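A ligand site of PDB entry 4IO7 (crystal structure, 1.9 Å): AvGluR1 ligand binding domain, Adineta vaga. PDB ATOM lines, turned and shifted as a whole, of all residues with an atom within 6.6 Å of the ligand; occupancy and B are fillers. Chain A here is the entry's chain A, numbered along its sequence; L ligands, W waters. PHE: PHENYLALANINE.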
ATOM      1  N   SER A  17     -25.528 -21.135 -31.899  1.00  0.00           N
ATOM      2  CA  SER A  17     -25.018 -19.861 -31.420  1.00  0.00           C
ATOM      3  C   SER A  17     -25.428 -18.788 -32.412  1.00  0.00           C
ATOM      4  O   SER A  17     -24.820 -18.660 -33.487  1.00  0.00           O
ATOM      5  CB  SER A  17     -23.484 -19.909 -31.295  1.00  0.00           C
ATOM      6  OG  SER A  17     -23.010 -18.674 -30.746  1.00  0.00           O
ATOM      7  N   TYR A  67     -18.587 -25.771 -25.553  1.00  0.00           N
ATOM      8  CA  TYR A  67     -17.554 -25.636 -26.562  1.00  0.00           C
ATOM      9  C   TYR A  67     -16.408 -26.592 -26.319  1.00  0.00           C
ATOM     10  O   TYR A  67     -15.871 -27.178 -27.255  1.00  0.00           O
ATOM     11  CB  TYR A  67     -17.102 -24.172 -26.654  1.00  0.00           C
ATOM     12  CG  TYR A  67     -18.137 -23.369 -27.389  1.00  0.00           C
ATOM     13  CD1 TYR A  67     -19.328 -23.033 -26.773  1.00  0.00           C
ATOM     14  CD2 TYR A  67     -17.936 -22.989 -28.708  1.00  0.00           C
ATOM     15  CE1 TYR A  67     -20.302 -22.315 -27.453  1.00  0.00           C
ATOM     16  CE2 TYR A  67     -18.908 -22.282 -29.390  1.00  0.00           C
ATOM     17  CZ  TYR A  67     -20.077 -21.950 -28.771  1.00  0.00           C
ATOM     18  OH  TYR A  67     -21.052 -21.262 -29.466  1.00  0.00           O
ATOM     19  N   THR A  68     -16.034 -26.754 -25.048  1.00  0.00           N
ATOM     20  CA  THR A  68     -15.033 -27.764 -24.693  1.00  0.00           C
ATOM     21  C   THR A  68     -15.540 -29.150 -25.110  1.00  0.00           C
ATOM     22  O   THR A  68     -14.777 -29.975 -25.632  1.00  0.00           O
ATOM     23  CB  THR A  68     -14.708 -27.690 -23.181  1.00  0.00           C
ATOM     24  OG1 THR A  68     -14.000 -26.476 -22.949  1.00  0.00           O
ATOM     25  CG2 THR A  68     -13.842 -28.872 -22.734  1.00  0.00           C
ATOM     26  N   ASP A  85     -18.159 -20.375 -33.723  1.00  0.00           N
ATOM     27  CA  ASP A  85     -17.488 -19.317 -32.959  1.00  0.00           C
ATOM     28  C   ASP A  85     -16.636 -19.987 -31.868  1.00  0.00           C
ATOM     29  O   ASP A  85     -16.917 -19.858 -30.687  1.00  0.00           O
ATOM     30  CB  ASP A  85     -18.522 -18.334 -32.357  1.00  0.00           C
ATOM     31  CG  ASP A  85     -19.723 -19.011 -31.666  1.00  0.00           C
ATOM     32  OD1 ASP A  85     -20.003 -20.239 -31.825  1.00  0.00           O
ATOM     33  OD2 ASP A  85     -20.433 -18.236 -30.980  1.00  0.00           O
ATOM     34  N   ILE A  86     -15.612 -20.717 -32.292  1.00  0.00           N
ATOM     35  CA  ILE A  86     -14.834 -21.576 -31.401  1.00  0.00           C
ATOM     36  C   ILE A  86     -13.474 -20.923 -31.168  1.00  0.00           C
ATOM     37  O   ILE A  86     -12.669 -20.775 -32.096  1.00  0.00           O
ATOM     38  CB  ILE A  86     -14.637 -22.981 -32.031  1.00  0.00           C
ATOM     39  CG1 ILE A  86     -15.984 -23.607 -32.360  1.00  0.00           C
ATOM     40  CG2 ILE A  86     -13.806 -23.902 -31.122  1.00  0.00           C
ATOM     41  CD1 ILE A  86     -15.843 -24.852 -33.268  1.00  0.00           C
ATOM     42  N   THR A  87     -13.223 -20.531 -29.919  1.00  0.00           N
ATOM     43  CA  THR A  87     -12.016 -19.795 -29.592  1.00  0.00           C
ATOM     44  C   THR A  87     -10.812 -20.731 -29.615  1.00  0.00           C
ATOM     45  O   THR A  87     -10.842 -21.824 -29.074  1.00  0.00           O
ATOM     46  CB  THR A  87     -12.160 -19.119 -28.262  1.00  0.00           C
ATOM     47  OG1 THR A  87     -13.321 -18.271 -28.351  1.00  0.00           O
ATOM     48  CG2 THR A  87     -10.919 -18.299 -27.884  1.00  0.00           C
ATOM     49  N   VAL A  88      -9.758 -20.247 -30.239  1.00  0.00           N
ATOM     50  CA  VAL A  88      -8.486 -20.965 -30.284  1.00  0.00           C
ATOM     51  C   VAL A  88      -7.765 -20.746 -28.933  1.00  0.00           C
ATOM     52  O   VAL A  88      -7.506 -19.617 -28.548  1.00  0.00           O
ATOM     53  CB  VAL A  88      -7.616 -20.415 -31.429  1.00  0.00           C
ATOM     54  CG1 VAL A  88      -6.260 -21.131 -31.481  1.00  0.00           C
ATOM     55  CG2 VAL A  88      -8.360 -20.495 -32.770  1.00  0.00           C
ATOM     56  N   THR A  89      -7.487 -21.809 -28.185  1.00  0.00           N
ATOM     57  CA  THR A  89      -6.820 -21.639 -26.881  1.00  0.00           C
ATOM     58  C   THR A  89      -5.686 -22.640 -26.792  1.00  0.00           C
ATOM     59  O   THR A  89      -5.703 -23.641 -27.497  1.00  0.00           O
ATOM     60  CB  THR A  89      -7.766 -21.891 -25.695  1.00  0.00           C
ATOM     61  OG1 THR A  89      -8.079 -23.292 -25.643  1.00  0.00           O
ATOM     62  CG2 THR A  89      -9.053 -21.077 -25.851  1.00  0.00           C
ATOM     63  N   ARG A  92      -6.913 -26.194 -25.764  1.00  0.00           N
ATOM     64  CA  ARG A  92      -7.521 -26.929 -26.861  1.00  0.00           C
ATOM     65  C   ARG A  92      -6.472 -27.404 -27.873  1.00  0.00           C
ATOM     66  O   ARG A  92      -6.582 -28.480 -28.441  1.00  0.00           O
ATOM     67  CB  ARG A  92      -8.570 -26.064 -27.547  1.00  0.00           C
ATOM     68  CG  ARG A  92      -9.725 -25.807 -26.590  1.00  0.00           C
ATOM     69  CD  ARG A  92     -10.699 -24.795 -27.135  1.00  0.00           C
ATOM     70  NE  ARG A  92     -11.762 -24.589 -26.163  1.00  0.00           N
ATOM     71  CZ  ARG A  92     -12.752 -23.739 -26.328  1.00  0.00           C
ATOM     72  NH1 ARG A  92     -12.800 -23.017 -27.420  1.00  0.00           N
ATOM     73  NH2 ARG A  92     -13.726 -23.636 -25.422  1.00  0.00           N
ATOM     74  N   ASN A 105     -11.467 -12.066 -32.315  1.00  0.00           N
ATOM     75  CA  ASN A 105     -12.478 -12.137 -31.281  1.00  0.00           C
ATOM     76  C   ASN A 105     -11.954 -11.422 -30.046  1.00  0.00           C
ATOM     77  O   ASN A 105     -10.757 -11.229 -29.879  1.00  0.00           O
ATOM     78  CB  ASN A 105     -12.776 -13.615 -30.943  1.00  0.00           C
ATOM     79  CG  ASN A 105     -13.896 -13.772 -29.941  1.00  0.00           C
ATOM     80  OD1 ASN A 105     -14.975 -13.203 -30.119  1.00  0.00           O
ATOM     81  ND2 ASN A 105     -13.653 -14.543 -28.880  1.00  0.00           N
ATOM     82  N   MET A 107     -13.763 -10.696 -25.706  1.00  0.00           N
ATOM     83  CA  MET A 107     -14.932 -10.740 -24.857  1.00  0.00           C
ATOM     84  C   MET A 107     -15.313  -9.409 -24.268  1.00  0.00           C
ATOM     85  O   MET A 107     -14.498  -8.487 -24.133  1.00  0.00           O
ATOM     86  CB  MET A 107     -14.700 -11.770 -23.751  1.00  0.00           C
ATOM     87  CG  MET A 107     -14.766 -13.217 -24.265  1.00  0.00           C
ATOM     88  SD  MET A 107     -14.788 -14.441 -22.914  1.00  0.00           S
ATOM     89  CE  MET A 107     -13.053 -14.547 -22.522  1.00  0.00           C
ATOM     90  N   ARG A 136     -20.489 -19.274 -18.425  1.00  0.00           N
ATOM     91  CA  ARG A 136     -20.871 -20.456 -19.187  1.00  0.00           C
ATOM     92  C   ARG A 136     -19.760 -21.494 -19.098  1.00  0.00           C
ATOM     93  O   ARG A 136     -18.634 -21.258 -19.530  1.00  0.00           O
ATOM     94  CB  ARG A 136     -21.174 -20.094 -20.638  1.00  0.00           C
ATOM     95  CG  ARG A 136     -21.410 -21.304 -21.526  1.00  0.00           C
ATOM     96  CD  ARG A 136     -22.838 -21.397 -22.020  1.00  0.00           C
ATOM     97  NE  ARG A 136     -22.960 -22.481 -23.001  1.00  0.00           N
ATOM     98  CZ  ARG A 136     -22.976 -22.334 -24.324  1.00  0.00           C
ATOM     99  NH1 ARG A 136     -22.907 -21.136 -24.870  1.00  0.00           N
ATOM    100  NH2 ARG A 136     -23.100 -23.405 -25.098  1.00  0.00           N
ATOM    101  N   GLY A 138     -17.320 -24.684 -19.731  1.00  0.00           N
ATOM    102  CA  GLY A 138     -16.714 -25.270 -20.913  1.00  0.00           C
ATOM    103  C   GLY A 138     -16.539 -24.268 -22.033  1.00  0.00           C
ATOM    104  O   GLY A 138     -16.616 -24.603 -23.224  1.00  0.00           O
ATOM    105  N   THR A 139     -16.254 -23.029 -21.646  1.00  0.00           N
ATOM    106  CA  THR A 139     -15.973 -21.978 -22.618  1.00  0.00           C
ATOM    107  C   THR A 139     -14.716 -21.251 -22.213  1.00  0.00           C
ATOM    108  O   THR A 139     -14.230 -21.363 -21.090  1.00  0.00           O
ATOM    109  CB  THR A 139     -17.096 -20.920 -22.726  1.00  0.00           C
ATOM    110  OG1 THR A 139     -17.193 -20.188 -21.491  1.00  0.00           O
ATOM    111  CG2 THR A 139     -18.429 -21.579 -23.089  1.00  0.00           C
ATOM    112  N   ALA A 140     -14.213 -20.470 -23.147  1.00  0.00           N
ATOM    113  CA  ALA A 140     -13.052 -19.628 -22.922  1.00  0.00           C
ATOM    114  C   ALA A 140     -13.304 -18.592 -21.841  1.00  0.00           C
ATOM    115  O   ALA A 140     -12.362 -18.117 -21.181  1.00  0.00           O
ATOM    116  CB  ALA A 140     -12.637 -18.965 -24.230  1.00  0.00           C
ATOM    117  N   GLY A 141     -14.556 -18.236 -21.632  1.00  0.00           N
ATOM    118  CA  GLY A 141     -14.901 -17.350 -20.541  1.00  0.00           C
ATOM    119  C   GLY A 141     -14.577 -17.954 -19.181  1.00  0.00           C
ATOM    120  O   GLY A 141     -14.126 -17.233 -18.275  1.00  0.00           O
ATOM    121  N   ASP A 143     -12.294 -20.227 -18.597  1.00  0.00           N
ATOM    122  CA  ASP A 143     -10.844 -20.254 -18.553  1.00  0.00           C
ATOM    123  C   ASP A 143     -10.306 -18.895 -18.106  1.00  0.00           C
ATOM    124  O   ASP A 143      -9.415 -18.802 -17.264  1.00  0.00           O
ATOM    125  CB  ASP A 143     -10.239 -20.574 -19.935  1.00  0.00           C
ATOM    126  CG  ASP A 143     -10.742 -21.902 -20.546  1.00  0.00           C
ATOM    127  OD1 ASP A 143     -11.238 -22.795 -19.836  1.00  0.00           O
ATOM    128  OD2 ASP A 143     -10.611 -22.050 -21.795  1.00  0.00           O
ATOM    129  N   ARG A 162     -26.780 -20.544 -23.502  1.00  0.00           N
ATOM    130  CA  ARG A 162     -26.898 -19.127 -23.720  1.00  0.00           C
ATOM    131  C   ARG A 162     -28.214 -18.682 -23.073  1.00  0.00           C
ATOM    132  O   ARG A 162     -28.269 -17.639 -22.423  1.00  0.00           O
ATOM    133  CB  ARG A 162     -26.866 -18.807 -25.230  1.00  0.00           C
ATOM    134  CG  ARG A 162     -26.206 -17.483 -25.581  1.00  0.00           C
ATOM    135  CD  ARG A 162     -25.619 -17.445 -27.025  1.00  0.00           C
ATOM    136  NE  ARG A 162     -24.343 -18.160 -27.151  1.00  0.00           N
ATOM    137  CZ  ARG A 162     -24.210 -19.424 -27.561  1.00  0.00           C
ATOM    138  NH1 ARG A 162     -25.282 -20.168 -27.878  1.00  0.00           N
ATOM    139  NH2 ARG A 162     -22.987 -19.953 -27.631  1.00  0.00           N
ATOM    140  N   MET A 165     -28.122 -18.087 -19.430  1.00  0.00           N
ATOM    141  CA  MET A 165     -27.487 -16.801 -19.175  1.00  0.00           C
ATOM    142  C   MET A 165     -28.456 -15.628 -19.301  1.00  0.00           C
ATOM    143  O   MET A 165     -28.451 -14.744 -18.444  1.00  0.00           O
ATOM    144  CB  MET A 165     -26.343 -16.549 -20.146  1.00  0.00           C
ATOM    145  CG  MET A 165     -25.718 -15.187 -19.931  1.00  0.00           C
ATOM    146  SD  MET A 165     -24.788 -14.712 -21.409  1.00  0.00           S
ATOM    147  CE  MET A 165     -23.282 -15.579 -21.136  1.00  0.00           C
ATOM    148  N   PHE A 178     -20.048 -12.959 -19.186  1.00  0.00           N
ATOM    149  CA  PHE A 178     -19.056 -12.692 -20.250  1.00  0.00           C
ATOM    150  C   PHE A 178     -19.592 -13.268 -21.534  1.00  0.00           C
ATOM    151  O   PHE A 178     -20.178 -14.348 -21.528  1.00  0.00           O
ATOM    152  CB  PHE A 178     -17.734 -13.428 -19.992  1.00  0.00           C
ATOM    153  CG  PHE A 178     -16.988 -12.999 -18.754  1.00  0.00           C
ATOM    154  CD1 PHE A 178     -17.287 -11.813 -18.096  1.00  0.00           C
ATOM    155  CD2 PHE A 178     -15.941 -13.787 -18.260  1.00  0.00           C
ATOM    156  CE1 PHE A 178     -16.585 -11.436 -16.945  1.00  0.00           C
ATOM    157  CE2 PHE A 178     -15.220 -13.405 -17.105  1.00  0.00           C
ATOM    158  CZ  PHE A 178     -15.534 -12.231 -16.462  1.00  0.00           C
ATOM    159  N   MET A 179     -19.379 -12.569 -22.651  1.00  0.00           N
ATOM    160  CA  MET A 179     -19.720 -13.113 -23.950  1.00  0.00           C
ATOM    161  C   MET A 179     -18.715 -12.617 -24.981  1.00  0.00           C
ATOM    162  O   MET A 179     -18.190 -11.496 -24.876  1.00  0.00           O
ATOM    163  CB  MET A 179     -21.087 -12.642 -24.416  1.00  0.00           C
ATOM    164  CG  MET A 179     -22.222 -13.671 -24.445  1.00  0.00           C
ATOM    165  SD  MET A 179     -23.747 -12.928 -25.061  1.00  0.00           S
ATOM    166  CE  MET A 179     -23.894 -13.800 -26.646  1.00  0.00           C
ATOM    167  N   ASP A 180     -18.475 -13.438 -25.984  1.00  0.00           N
ATOM    168  CA  ASP A 180     -17.756 -12.975 -27.168  1.00  0.00           C
ATOM    169  C   ASP A 180     -18.452 -11.741 -27.744  1.00  0.00           C
ATOM    170  O   ASP A 180     -19.696 -11.617 -27.728  1.00  0.00           O
ATOM    171  CB  ASP A 180     -17.733 -14.059 -28.251  1.00  0.00           C
ATOM    172  CG  ASP A 180     -16.952 -15.289 -27.846  1.00  0.00           C
ATOM    173  OD1 ASP A 180     -16.038 -15.210 -27.003  1.00  0.00           O
ATOM    174  OD2 ASP A 180     -17.275 -16.371 -28.386  1.00  0.00           O
ATOM    175  N   THR A 183     -21.303 -12.010 -30.911  1.00  0.00           N
ATOM    176  CA  THR A 183     -22.614 -12.480 -30.488  1.00  0.00           C
ATOM    177  C   THR A 183     -23.221 -11.601 -29.387  1.00  0.00           C
ATOM    178  O   THR A 183     -24.450 -11.461 -29.305  1.00  0.00           O
ATOM    179  CB  THR A 183     -22.574 -13.923 -29.999  1.00  0.00           C
ATOM    180  OG1 THR A 183     -21.451 -14.126 -29.143  1.00  0.00           O
ATOM    181  CG2 THR A 183     -22.493 -14.882 -31.204  1.00  0.00           C
ATOM    182  N   ALA A 184     -22.369 -11.016 -28.557  1.00  0.00           N
ATOM    183  CA  ALA A 184     -22.856 -10.108 -27.515  1.00  0.00           C
ATOM    184  C   ALA A 184     -23.524  -8.889 -28.161  1.00  0.00           C
ATOM    185  O   ALA A 184     -24.620  -8.480 -27.743  1.00  0.00           O
ATOM    186  CB  ALA A 184     -21.720  -9.654 -26.643  1.00  0.00           C
ATOM    187  N   PHE A 207     -11.100 -17.027 -33.664  1.00  0.00           N
ATOM    188  CA  PHE A 207     -11.889 -18.242 -33.961  1.00  0.00           C
ATOM    189  C   PHE A 207     -11.210 -19.018 -35.073  1.00  0.00           C
ATOM    190  O   PHE A 207     -10.722 -18.414 -36.041  1.00  0.00           O
ATOM    191  CB  PHE A 207     -13.306 -17.896 -34.446  1.00  0.00           C
ATOM    192  CG  PHE A 207     -14.180 -17.189 -33.427  1.00  0.00           C
ATOM    193  CD1 PHE A 207     -14.079 -17.465 -32.064  1.00  0.00           C
ATOM    194  CD2 PHE A 207     -15.146 -16.276 -33.845  1.00  0.00           C
ATOM    195  CE1 PHE A 207     -14.922 -16.851 -31.150  1.00  0.00           C
ATOM    196  CE2 PHE A 207     -15.977 -15.628 -32.923  1.00  0.00           C
ATOM    197  CZ  PHE A 207     -15.872 -15.913 -31.571  1.00  0.00           C
HETATM  198  N   PHE L   1     -16.144 -18.769 -28.073  1.00  0.00           N
HETATM  199  CA  PHE L   1     -16.364 -19.494 -26.777  1.00  0.00           C
HETATM  200  C   PHE L   1     -15.498 -20.705 -26.725  1.00  0.00           C
HETATM  201  O   PHE L   1     -14.993 -21.149 -27.774  1.00  0.00           O
HETATM  202  CB  PHE L   1     -17.809 -19.959 -26.640  1.00  0.00           C
HETATM  203  CG  PHE L   1     -18.788 -18.832 -26.601  1.00  0.00           C
HETATM  204  CD1 PHE L   1     -18.890 -18.035 -25.468  1.00  0.00           C
HETATM  205  CD2 PHE L   1     -19.616 -18.572 -27.699  1.00  0.00           C
HETATM  206  CE1 PHE L   1     -19.804 -16.964 -25.429  1.00  0.00           C
HETATM  207  CE2 PHE L   1     -20.534 -17.509 -27.682  1.00  0.00           C
HETATM  208  CZ  PHE L   1     -20.621 -16.687 -26.553  1.00  0.00           C
HETATM  209  OXT PHE L   1     -15.342 -21.235 -25.614  1.00  0.00           O
HETATM  210  O   HOH W   1     -18.236 -17.563 -22.150  1.00  0.00           O
HETATM  211  O   HOH W   2     -16.384 -17.025 -24.091  1.00  0.00           O
HETATM  212  O   HOH W   3     -19.464 -15.886 -30.115  1.00  0.00           O
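A nitrogen (N) of the ligand is in salt-bridge range of the side-chain carboxylate (OD2) of Asp 180 (2.7 Å).
The backbone NH (N) of Ala 140 lies within hydrogen-bond range of an oxygen (OXT) of the ligand (2.8 Å).
N of Thr 87 sits at hydrogen-bond distance from O of the ligand (2.8 Å).
N of the ligand is in hydrogen-bond range of OG1 of Thr 87 (2.9 Å).
The guanidinium group (NH2) of Arg 92 lies within salt-bridge range of an oxygen (OXT) of the ligand (2.9 Å).
The backbone carbonyl oxygen (O) of Asp 85 sits at hydrogen-bond distance from a nitrogen (N) of the ligand (2.9 Å).
Residues that only touch the ligand: Tyr 67, Ile 86, Thr 139, Arg 162, Thr 183 and Phe 207.
Hydrophobic or aromatic side chains within 4 Å of the ligand: Tyr 67, Ala 140 and Phe 207.
Of the 25 residues printed, 11 come within 4 Å of the ligand.
The nearest printed residue that does not touch the ligand is Met 179 (4.01 Å).
O of Asp 180 is in hydrogen-bond range of OG1 of Thr 183 (3.4 Å).
OD1 of Asp 180 is in hydrogen-bond range of ND2 of Asn 105, 3.1 Å away.
The backbone carbonyl oxygen of Thr 87 lies within hydrogen-bond range of the guanidinium group of Arg 92 (2.8 Å).
The side-chain hydroxyl (OG1) of Thr 89 sits at hydrogen-bond distance from the backbone NH (N) of Arg 92 (3.1 Å).
OG of Ser 17 is in hydrogen-bond range of OD2 of Asp 85 (2.6 Å).
The side-chain hydroxyl (OG1) of Thr 139 lies within hydrogen-bond range of the backbone carbonyl oxygen (O) of Arg 136, 2.7 Å away.
OH of Tyr 67 lies close to OG of Ser 17 (3.5 Å).
The backbone carbonyl oxygen (O) of Gly 138 sits at hydrogen-bond distance from the backbone NH (N) of Tyr 67, at 3.3 Å.
Water W2 lies within hydrogen-bond range of SD of Met 107 (3.3 Å), N of Gly 141 (3.3 Å) and OD1 of Asp 180 (3.4 Å).
Water W3 lies within hydrogen-bond range of the side-chain carboxylate of Asp 85, the side-chain hydroxyl of Thr 183 and the side-chain carboxylate of Asp 180.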
